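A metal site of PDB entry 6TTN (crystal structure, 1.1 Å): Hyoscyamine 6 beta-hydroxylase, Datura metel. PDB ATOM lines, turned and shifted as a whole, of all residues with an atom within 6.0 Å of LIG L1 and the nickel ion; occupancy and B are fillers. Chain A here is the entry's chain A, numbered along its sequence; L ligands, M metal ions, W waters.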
ATOM      1  N   GLU A  86      -8.685  18.992  -3.723  1.00  0.00           N
ATOM      2  CA  GLU A  86      -9.477  18.590  -2.567  1.00  0.00           C
ATOM      3  C   GLU A  86      -8.616  17.718  -1.688  1.00  0.00           C
ATOM      4  O   GLU A  86      -8.115  16.695  -2.153  1.00  0.00           O
ATOM      5  CB  GLU A  86     -10.708  17.803  -3.039  1.00  0.00           C
ATOM      6  CG  GLU A  86     -11.761  17.577  -1.945  1.00  0.00           C
ATOM      7  CD  GLU A  86     -13.008  16.833  -2.390  1.00  0.00           C
ATOM      8  OE1 GLU A  86     -13.034  16.311  -3.508  1.00  0.00           O
ATOM      9  OE2 GLU A  86     -13.986  16.792  -1.618  1.00  0.00           O
ATOM     10  N   LYS A  99      -5.356  14.478  -6.000  1.00  0.00           N
ATOM     11  CA  LYS A  99      -6.509  14.448  -6.884  1.00  0.00           C
ATOM     12  C   LYS A  99      -6.708  15.799  -7.553  1.00  0.00           C
ATOM     13  O   LYS A  99      -6.850  16.824  -6.884  1.00  0.00           O
ATOM     14  CB  LYS A  99      -7.798  14.097  -6.118  1.00  0.00           C
ATOM     15  CG  LYS A  99      -9.049  14.029  -7.036  1.00  0.00           C
ATOM     16  CD  LYS A  99     -10.303  13.514  -6.312  1.00  0.00           C
ATOM     17  CE  LYS A  99     -10.841  14.431  -5.210  1.00  0.00           C
ATOM     18  NZ  LYS A  99     -11.652  15.551  -5.720  1.00  0.00           N
ATOM     19  N   LEU A 168     -17.696  15.525 -12.640  1.00  0.00           N
ATOM     20  CA  LEU A 168     -16.420  15.613 -11.933  1.00  0.00           C
ATOM     21  C   LEU A 168     -15.513  14.556 -12.547  1.00  0.00           C
ATOM     22  O   LEU A 168     -15.708  13.357 -12.305  1.00  0.00           O
ATOM     23  CB  LEU A 168     -16.552  15.369 -10.433  1.00  0.00           C
ATOM     24  CG  LEU A 168     -16.959  16.563  -9.556  1.00  0.00           C
ATOM     25  CD1 LEU A 168     -18.278  17.173  -9.948  1.00  0.00           C
ATOM     26  CD2 LEU A 168     -16.947  16.201  -8.089  1.00  0.00           C
ATOM     27  N   ASN A 170     -11.932  13.030 -12.490  1.00  0.00           N
ATOM     28  CA  ASN A 170     -10.886  12.994 -11.482  1.00  0.00           C
ATOM     29  C   ASN A 170      -9.634  12.326 -12.028  1.00  0.00           C
ATOM     30  O   ASN A 170      -9.707  11.276 -12.657  1.00  0.00           O
ATOM     31  CB  ASN A 170     -11.362  12.150 -10.302  1.00  0.00           C
ATOM     32  CG  ASN A 170     -12.706  12.603  -9.814  1.00  0.00           C
ATOM     33  OD1 ASN A 170     -12.873  13.746  -9.398  1.00  0.00           O
ATOM     34  ND2 ASN A 170     -13.691  11.723  -9.935  1.00  0.00           N
ATOM     35  N   TYR A 172      -5.952  10.995 -10.578  1.00  0.00           N
ATOM     36  CA  TYR A 172      -5.227  10.591  -9.358  1.00  0.00           C
ATOM     37  C   TYR A 172      -3.813  10.237  -9.773  1.00  0.00           C
ATOM     38  O   TYR A 172      -3.575   9.146 -10.289  1.00  0.00           O
ATOM     39  CB  TYR A 172      -5.897   9.372  -8.718  1.00  0.00           C
ATOM     40  CG  TYR A 172      -7.333   9.609  -8.312  1.00  0.00           C
ATOM     41  CD1 TYR A 172      -7.630  10.115  -7.064  1.00  0.00           C
ATOM     42  CD2 TYR A 172      -8.374   9.241  -9.147  1.00  0.00           C
ATOM     43  CE1 TYR A 172      -8.956  10.341  -6.679  1.00  0.00           C
ATOM     44  CE2 TYR A 172      -9.712   9.440  -8.774  1.00  0.00           C
ATOM     45  CZ  TYR A 172      -9.993   9.961  -7.526  1.00  0.00           C
ATOM     46  OH  TYR A 172     -11.279  10.186  -7.110  1.00  0.00           O
ATOM     47  N   HIS A 187     -16.316   9.335   2.201  1.00  0.00           N
ATOM     48  CA  HIS A 187     -17.361  10.339   2.175  1.00  0.00           C
ATOM     49  C   HIS A 187     -18.647   9.713   1.665  1.00  0.00           C
ATOM     50  O   HIS A 187     -18.637   8.723   0.933  1.00  0.00           O
ATOM     51  CB  HIS A 187     -16.990  11.533   1.262  1.00  0.00           C
ATOM     52  CG  HIS A 187     -16.790  11.155  -0.178  1.00  0.00           C
ATOM     53  ND1 HIS A 187     -15.616  10.629  -0.663  1.00  0.00           N
ATOM     54  CD2 HIS A 187     -17.627  11.183  -1.238  1.00  0.00           C
ATOM     55  CE1 HIS A 187     -15.753  10.323  -1.945  1.00  0.00           C
ATOM     56  NE2 HIS A 187     -16.973  10.683  -2.326  1.00  0.00           N
ATOM     57  N   TYR A 188     -19.770  10.326   2.052  1.00  0.00           N
ATOM     58  CA  TYR A 188     -20.971  10.260   1.215  1.00  0.00           C
ATOM     59  C   TYR A 188     -20.855  11.335   0.137  1.00  0.00           C
ATOM     60  O   TYR A 188     -20.283  12.405   0.401  1.00  0.00           O
ATOM     61  CB  TYR A 188     -22.227  10.671   1.984  1.00  0.00           C
ATOM     62  CG  TYR A 188     -22.734   9.803   3.108  1.00  0.00           C
ATOM     63  CD1 TYR A 188     -23.517   8.694   2.858  1.00  0.00           C
ATOM     64  CD2 TYR A 188     -22.488  10.147   4.429  1.00  0.00           C
ATOM     65  CE1 TYR A 188     -24.027   7.947   3.890  1.00  0.00           C
ATOM     66  CE2 TYR A 188     -22.987   9.409   5.456  1.00  0.00           C
ATOM     67  CZ  TYR A 188     -23.766   8.302   5.198  1.00  0.00           C
ATOM     68  OH  TYR A 188     -24.309   7.538   6.232  1.00  0.00           O
ATOM     69  N   ASP A 189     -21.409  11.085  -1.052  1.00  0.00           N
ATOM     70  CA  ASP A 189     -21.677  12.190  -1.960  1.00  0.00           C
ATOM     71  C   ASP A 189     -22.887  12.924  -1.409  1.00  0.00           C
ATOM     72  O   ASP A 189     -23.846  12.311  -0.963  1.00  0.00           O
ATOM     73  CB  ASP A 189     -21.991  11.678  -3.372  1.00  0.00           C
ATOM     74  CG  ASP A 189     -20.816  11.027  -4.075  1.00  0.00           C
ATOM     75  OD1 ASP A 189     -19.658  11.076  -3.561  1.00  0.00           O
ATOM     76  OD2 ASP A 189     -21.056  10.488  -5.186  1.00  0.00           O
ATOM     77  N   THR A 194     -25.307   9.505  -7.856  1.00  0.00           N
ATOM     78  CA  THR A 194     -24.109   9.645  -8.667  1.00  0.00           C
ATOM     79  C   THR A 194     -23.896   8.403  -9.501  1.00  0.00           C
ATOM     80  O   THR A 194     -24.074   7.281  -9.024  1.00  0.00           O
ATOM     81  CB  THR A 194     -22.903   9.836  -7.748  1.00  0.00           C
ATOM     82  OG1 THR A 194     -23.111  11.008  -6.954  1.00  0.00           O
ATOM     83  CG2 THR A 194     -21.583   9.914  -8.530  1.00  0.00           C
ATOM     84  N   LEU A 196     -20.757   6.717 -11.751  1.00  0.00           N
ATOM     85  CA  LEU A 196     -19.313   6.815 -11.853  1.00  0.00           C
ATOM     86  C   LEU A 196     -18.793   5.774 -12.850  1.00  0.00           C
ATOM     87  O   LEU A 196     -19.115   4.588 -12.756  1.00  0.00           O
ATOM     88  CB  LEU A 196     -18.694   6.595 -10.482  1.00  0.00           C
ATOM     89  CG  LEU A 196     -17.177   6.778 -10.537  1.00  0.00           C
ATOM     90  CD1 LEU A 196     -16.703   8.129 -10.159  1.00  0.00           C
ATOM     91  CD2 LEU A 196     -16.392   5.649  -9.939  1.00  0.00           C
ATOM     92  N   GLN A 198     -15.377   4.013 -14.238  1.00  0.00           N
ATOM     93  CA  GLN A 198     -13.999   3.712 -13.868  1.00  0.00           C
ATOM     94  C   GLN A 198     -13.484   2.543 -14.687  1.00  0.00           C
ATOM     95  O   GLN A 198     -14.247   1.705 -15.158  1.00  0.00           O
ATOM     96  CB  GLN A 198     -13.869   3.378 -12.383  1.00  0.00           C
ATOM     97  CG  GLN A 198     -14.727   2.216 -11.953  1.00  0.00           C
ATOM     98  CD  GLN A 198     -14.384   1.590 -10.633  1.00  0.00           C
ATOM     99  OE1 GLN A 198     -13.435   2.000  -9.967  1.00  0.00           O
ATOM    100  NE2 GLN A 198     -15.160   0.604 -10.251  1.00  0.00           N
ATOM    101  N   GLY A 202      -9.435   1.001  -7.359  1.00  0.00           N
ATOM    102  CA  GLY A 202      -9.181   2.114  -6.479  1.00  0.00           C
ATOM    103  C   GLY A 202     -10.390   2.510  -5.647  1.00  0.00           C
ATOM    104  O   GLY A 202     -10.234   3.090  -4.565  1.00  0.00           O
ATOM    105  N   LEU A 203     -11.599   2.244  -6.122  1.00  0.00           N
ATOM    106  CA  LEU A 203     -12.802   2.604  -5.377  1.00  0.00           C
ATOM    107  C   LEU A 203     -13.136   1.525  -4.368  1.00  0.00           C
ATOM    108  O   LEU A 203     -13.168   0.337  -4.697  1.00  0.00           O
ATOM    109  CB  LEU A 203     -13.960   2.788  -6.350  1.00  0.00           C
ATOM    110  CG  LEU A 203     -15.327   3.155  -5.761  1.00  0.00           C
ATOM    111  CD1 LEU A 203     -15.267   4.516  -5.061  1.00  0.00           C
ATOM    112  CD2 LEU A 203     -16.373   3.190  -6.872  1.00  0.00           C
ATOM    113  N   ASN A 226     -24.203   5.248  -6.968  1.00  0.00           N
ATOM    114  CA  ASN A 226     -24.218   5.387  -5.519  1.00  0.00           C
ATOM    115  C   ASN A 226     -25.215   6.445  -5.085  1.00  0.00           C
ATOM    116  O   ASN A 226     -25.403   7.484  -5.735  1.00  0.00           O
ATOM    117  CB  ASN A 226     -22.867   5.584  -4.906  1.00  0.00           C
ATOM    118  CG  ASN A 226     -22.250   6.840  -5.333  1.00  0.00           C
ATOM    119  OD1 ASN A 226     -21.583   6.884  -6.398  1.00  0.00           O
ATOM    120  ND2 ASN A 226     -22.349   7.889  -4.477  1.00  0.00           N
ATOM    121  N   HIS A 244     -17.958   5.849   0.621  1.00  0.00           N
ATOM    122  CA  HIS A 244     -16.962   5.243  -0.245  1.00  0.00           C
ATOM    123  C   HIS A 244     -15.688   6.075  -0.208  1.00  0.00           C
ATOM    124  O   HIS A 244     -15.670   7.204   0.281  1.00  0.00           O
ATOM    125  CB  HIS A 244     -17.522   5.048  -1.671  1.00  0.00           C
ATOM    126  CG  HIS A 244     -18.076   6.321  -2.257  1.00  0.00           C
ATOM    127  ND1 HIS A 244     -19.362   6.762  -2.042  1.00  0.00           N
ATOM    128  CD2 HIS A 244     -17.496   7.297  -2.985  1.00  0.00           C
ATOM    129  CE1 HIS A 244     -19.526   7.925  -2.634  1.00  0.00           C
ATOM    130  NE2 HIS A 244     -18.399   8.293  -3.208  1.00  0.00           N
ATOM    131  N   ARG A 245     -14.595   5.500  -0.711  1.00  0.00           N
ATOM    132  CA  ARG A 245     -13.298   6.160  -0.689  1.00  0.00           C
ATOM    133  C   ARG A 245     -12.484   5.695  -1.886  1.00  0.00           C
ATOM    134  O   ARG A 245     -12.801   4.681  -2.517  1.00  0.00           O
ATOM    135  CB  ARG A 245     -12.528   5.876   0.610  1.00  0.00           C
ATOM    136  CG  ARG A 245     -11.963   4.465   0.727  1.00  0.00           C
ATOM    137  CD  ARG A 245     -11.295   4.231   2.072  1.00  0.00           C
ATOM    138  NE  ARG A 245     -10.707   2.885   2.116  1.00  0.00           N
ATOM    139  CZ  ARG A 245     -10.193   2.339   3.208  1.00  0.00           C
ATOM    140  NH1 ARG A 245     -10.189   3.019   4.338  1.00  0.00           N
ATOM    141  NH2 ARG A 245      -9.680   1.113   3.148  1.00  0.00           N
ATOM    142  N   VAL A 246     -11.413   6.445  -2.173  1.00  0.00           N
ATOM    143  CA  VAL A 246     -10.535   6.105  -3.282  1.00  0.00           C
ATOM    144  C   VAL A 246      -9.120   5.871  -2.772  1.00  0.00           C
ATOM    145  O   VAL A 246      -8.577   6.685  -2.023  1.00  0.00           O
ATOM    146  CB  VAL A 246     -10.520   7.213  -4.353  1.00  0.00           C
ATOM    147  CG1 VAL A 246      -9.530   6.903  -5.481  1.00  0.00           C
ATOM    148  CG2 VAL A 246     -11.942   7.409  -4.888  1.00  0.00           C
ATOM    149  N   ARG A 254      -4.824   7.071 -12.357  1.00  0.00           N
ATOM    150  CA  ARG A 254      -6.212   6.656 -12.546  1.00  0.00           C
ATOM    151  C   ARG A 254      -7.116   7.843 -12.853  1.00  0.00           C
ATOM    152  O   ARG A 254      -6.988   8.900 -12.242  1.00  0.00           O
ATOM    153  CB  ARG A 254      -6.658   5.962 -11.264  1.00  0.00           C
ATOM    154  CG  ARG A 254      -8.100   5.472 -11.261  1.00  0.00           C
ATOM    155  CD  ARG A 254      -8.367   4.590 -10.050  1.00  0.00           C
ATOM    156  NE  ARG A 254      -9.746   4.155  -9.968  1.00  0.00           N
ATOM    157  CZ  ARG A 254     -10.742   4.884  -9.478  1.00  0.00           C
ATOM    158  NH1 ARG A 254     -10.497   6.082  -9.000  1.00  0.00           N
ATOM    159  NH2 ARG A 254     -11.983   4.439  -9.481  1.00  0.00           N
ATOM    160  N   SER A 256     -11.315   8.760 -13.260  1.00  0.00           N
ATOM    161  CA  SER A 256     -12.701   8.351 -13.140  1.00  0.00           C
ATOM    162  C   SER A 256     -13.583   9.512 -13.569  1.00  0.00           C
ATOM    163  O   SER A 256     -13.181  10.684 -13.515  1.00  0.00           O
ATOM    164  CB  SER A 256     -13.035   7.926 -11.728  1.00  0.00           C
ATOM    165  OG  SER A 256     -12.907   9.019 -10.867  1.00  0.00           O
ATOM    166  N   LEU A 260     -22.747  13.710 -10.936  1.00  0.00           N
ATOM    167  CA  LEU A 260     -23.348  13.910  -9.622  1.00  0.00           C
ATOM    168  C   LEU A 260     -24.606  14.750  -9.829  1.00  0.00           C
ATOM    169  O   LEU A 260     -24.533  15.952 -10.127  1.00  0.00           O
ATOM    170  CB  LEU A 260     -22.398  14.633  -8.673  1.00  0.00           C
ATOM    171  CG  LEU A 260     -21.264  13.793  -8.068  1.00  0.00           C
ATOM    172  CD1 LEU A 260     -20.212  13.386  -9.125  1.00  0.00           C
ATOM    173  CD2 LEU A 260     -20.632  14.552  -6.939  1.00  0.00           C
HETATM  174  C1  LIG L   1     -16.104  11.262  -5.861  1.00  0.00           C
HETATM  175  C2  LIG L   1     -15.762   9.814  -5.825  1.00  0.00           C
HETATM  176  C3  LIG L   1     -14.704   7.876  -6.823  1.00  0.00           C
HETATM  177  C4  LIG L   1     -13.609   7.577  -7.784  1.00  0.00           C
HETATM  178  O1  LIG L   1     -17.031  11.648  -5.174  1.00  0.00           O
HETATM  179  O2  LIG L   1     -15.408  12.021  -6.665  1.00  0.00           O
HETATM  180  O3  LIG L   1     -16.215   9.129  -4.909  1.00  0.00           O
HETATM  181  O4  LIG L   1     -12.944   8.471  -8.301  1.00  0.00           O
HETATM  182  N1  LIG L   1     -14.985   9.294  -6.793  1.00  0.00           N
HETATM  183  O5  LIG L   1     -13.444   6.322  -8.027  1.00  0.00           O
HETATM  184  C1  LG2 L   2     -16.500  17.136  -4.270  1.00  0.00           C
HETATM  185  C2  LG2 L   2     -19.440  18.235  -4.454  1.00  0.00           C
HETATM  186  C3  LG2 L   2     -21.788  18.499  -3.877  1.00  0.00           C
HETATM  187  C4  LG2 L   2     -22.927  17.710  -3.428  1.00  0.00           C
HETATM  188  C5  LG2 L   2     -22.555  20.424  -2.438  1.00  0.00           C
HETATM  189  C6  LG2 L   2     -23.706  19.623  -1.998  1.00  0.00           C
HETATM  190  C7  LG2 L   2     -17.058  15.115  -2.366  1.00  0.00           C
HETATM  191  C8  LG2 L   2     -16.224  15.652  -4.354  1.00  0.00           C
HETATM  192  C9  LG2 L   2     -18.071  14.476  -3.367  1.00  0.00           C
HETATM  193  C10 LG2 L   2     -17.529  14.860  -4.681  1.00  0.00           C
HETATM  194  C11 LG2 L   2     -17.451  16.513  -1.950  1.00  0.00           C
HETATM  195  C12 LG2 L   2     -17.646  17.486  -3.204  1.00  0.00           C
HETATM  196  C13 LG2 L   2     -15.233  13.814  -3.187  1.00  0.00           C
HETATM  197  C14 LG2 L   2     -20.850  17.929  -4.886  1.00  0.00           C
HETATM  198  C15 LG2 L   2     -21.186  18.538  -6.276  1.00  0.00           C
HETATM  199  C16 LG2 L   2     -21.604  19.872  -3.401  1.00  0.00           C
HETATM  200  C17 LG2 L   2     -23.893  18.259  -2.484  1.00  0.00           C
HETATM  201  N1  LG2 L   2     -15.865  15.098  -3.110  1.00  0.00           N
HETATM  202  O1  LG2 L   2     -18.904  17.259  -3.667  1.00  0.00           O
HETATM  203  O2  LG2 L   2     -18.813  19.229  -4.779  1.00  0.00           O
HETATM  204  O3  LG2 L   2     -22.551  18.285  -6.626  1.00  0.00           O
HETATM  205 NI    NI M   1     -17.898  10.081  -4.109  1.00  0.00          NI
HETATM  206  O   HOH W   1     -18.747   9.506  -5.985  1.00  0.00           O
HETATM  207  O   HOH W   2     -12.693  11.510  -5.119  1.00  0.00           O
HETATM  208  O   HOH W   3     -14.036  14.316  -6.966  1.00  0.00           O
HETATM  209  O   HOH W   4     -16.447  12.011  -9.555  1.00  0.00           O
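OG of Ser 256 sits at hydrogen-bond distance from O4 of LIG L1 (2.6 Å).
O4 of LIG L1 lies within hydrogen-bond range of OH of Tyr 172, at 2.7 Å.
The side-chain carboxylate (OE2) of Glu 86 lies within salt-bridge range of a nitrogen (N1) of LG2 L2, at 2.9 Å.
The guanidinium group (NH2) of Arg 254 is in salt-bridge range of an oxygen (O5) of LIG L1 (2.8 Å).
N of Asn 170 sits at hydrogen-bond distance from O of Ser 256 (2.8 Å).
The side-chain carboxylate (OD2) of Asp 189 is in hydrogen-bond range of the side-chain amide nitrogen (ND2) of Asn 226.
The side-chain hydroxyl (OG1) of Thr 194 lies within hydrogen-bond range of the side-chain carboxylate (OD2) of Asp 189.
The side-chain amide oxygen (OE1) of Gln 198 lies within hydrogen-bond range of the guanidinium group (NH2) of Arg 254 (2.9 Å).
The backbone carbonyl oxygen (O) of Arg 254 sits at hydrogen-bond distance from the backbone NH (N) of Tyr 172 (2.9 Å).
Merely in contact with LIG L1: Val 246 (3.3 Å), Leu 196 (3.6 Å), Asn 170 (3.7 Å) and Leu 203 (3.8 Å).
Along chain A the residues within 4 Å of the nickel ion span positions 187 to 244.
The nearest printed residue that does not touch the nickel ion is Asn 226 (5.0 Å).
NE2 of His 244 is bound to the nickel ion.
O1 of LIG L1 binds the nickel ion, at 2.1 Å.
O3 of LIG L1 binds the nickel ion, at 2.1 Å.
The nickel ion is bound by OD1 of Asp 189, at 2.1 Å.
A ring nitrogen (NE2) of His 187 is bound to the nickel ion.
Water W1 binds the nickel ion.
Water W3 lies within hydrogen-bond range of an oxygen (O2) of LIG L1 (2.7 Å), the side-chain amide oxygen (OD1) of Asn 170 (2.8 Å) and the side-chain amino group (NZ) of Lys 99 (3.0 Å).
Water W4 lies within hydrogen-bond range of the side-chain amide nitrogen (ND2) of Asn 170 (2.8 Å), an oxygen (O2) of LIG L1 (3.1 Å) and the backbone carbonyl oxygen (O) of Leu 168 (3.1 Å).
Water W2 lies within hydrogen-bond range of the side-chain hydroxyl of Tyr 172 (2.8 Å) and an oxygen (O2) of LIG L1 (3.2 Å).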
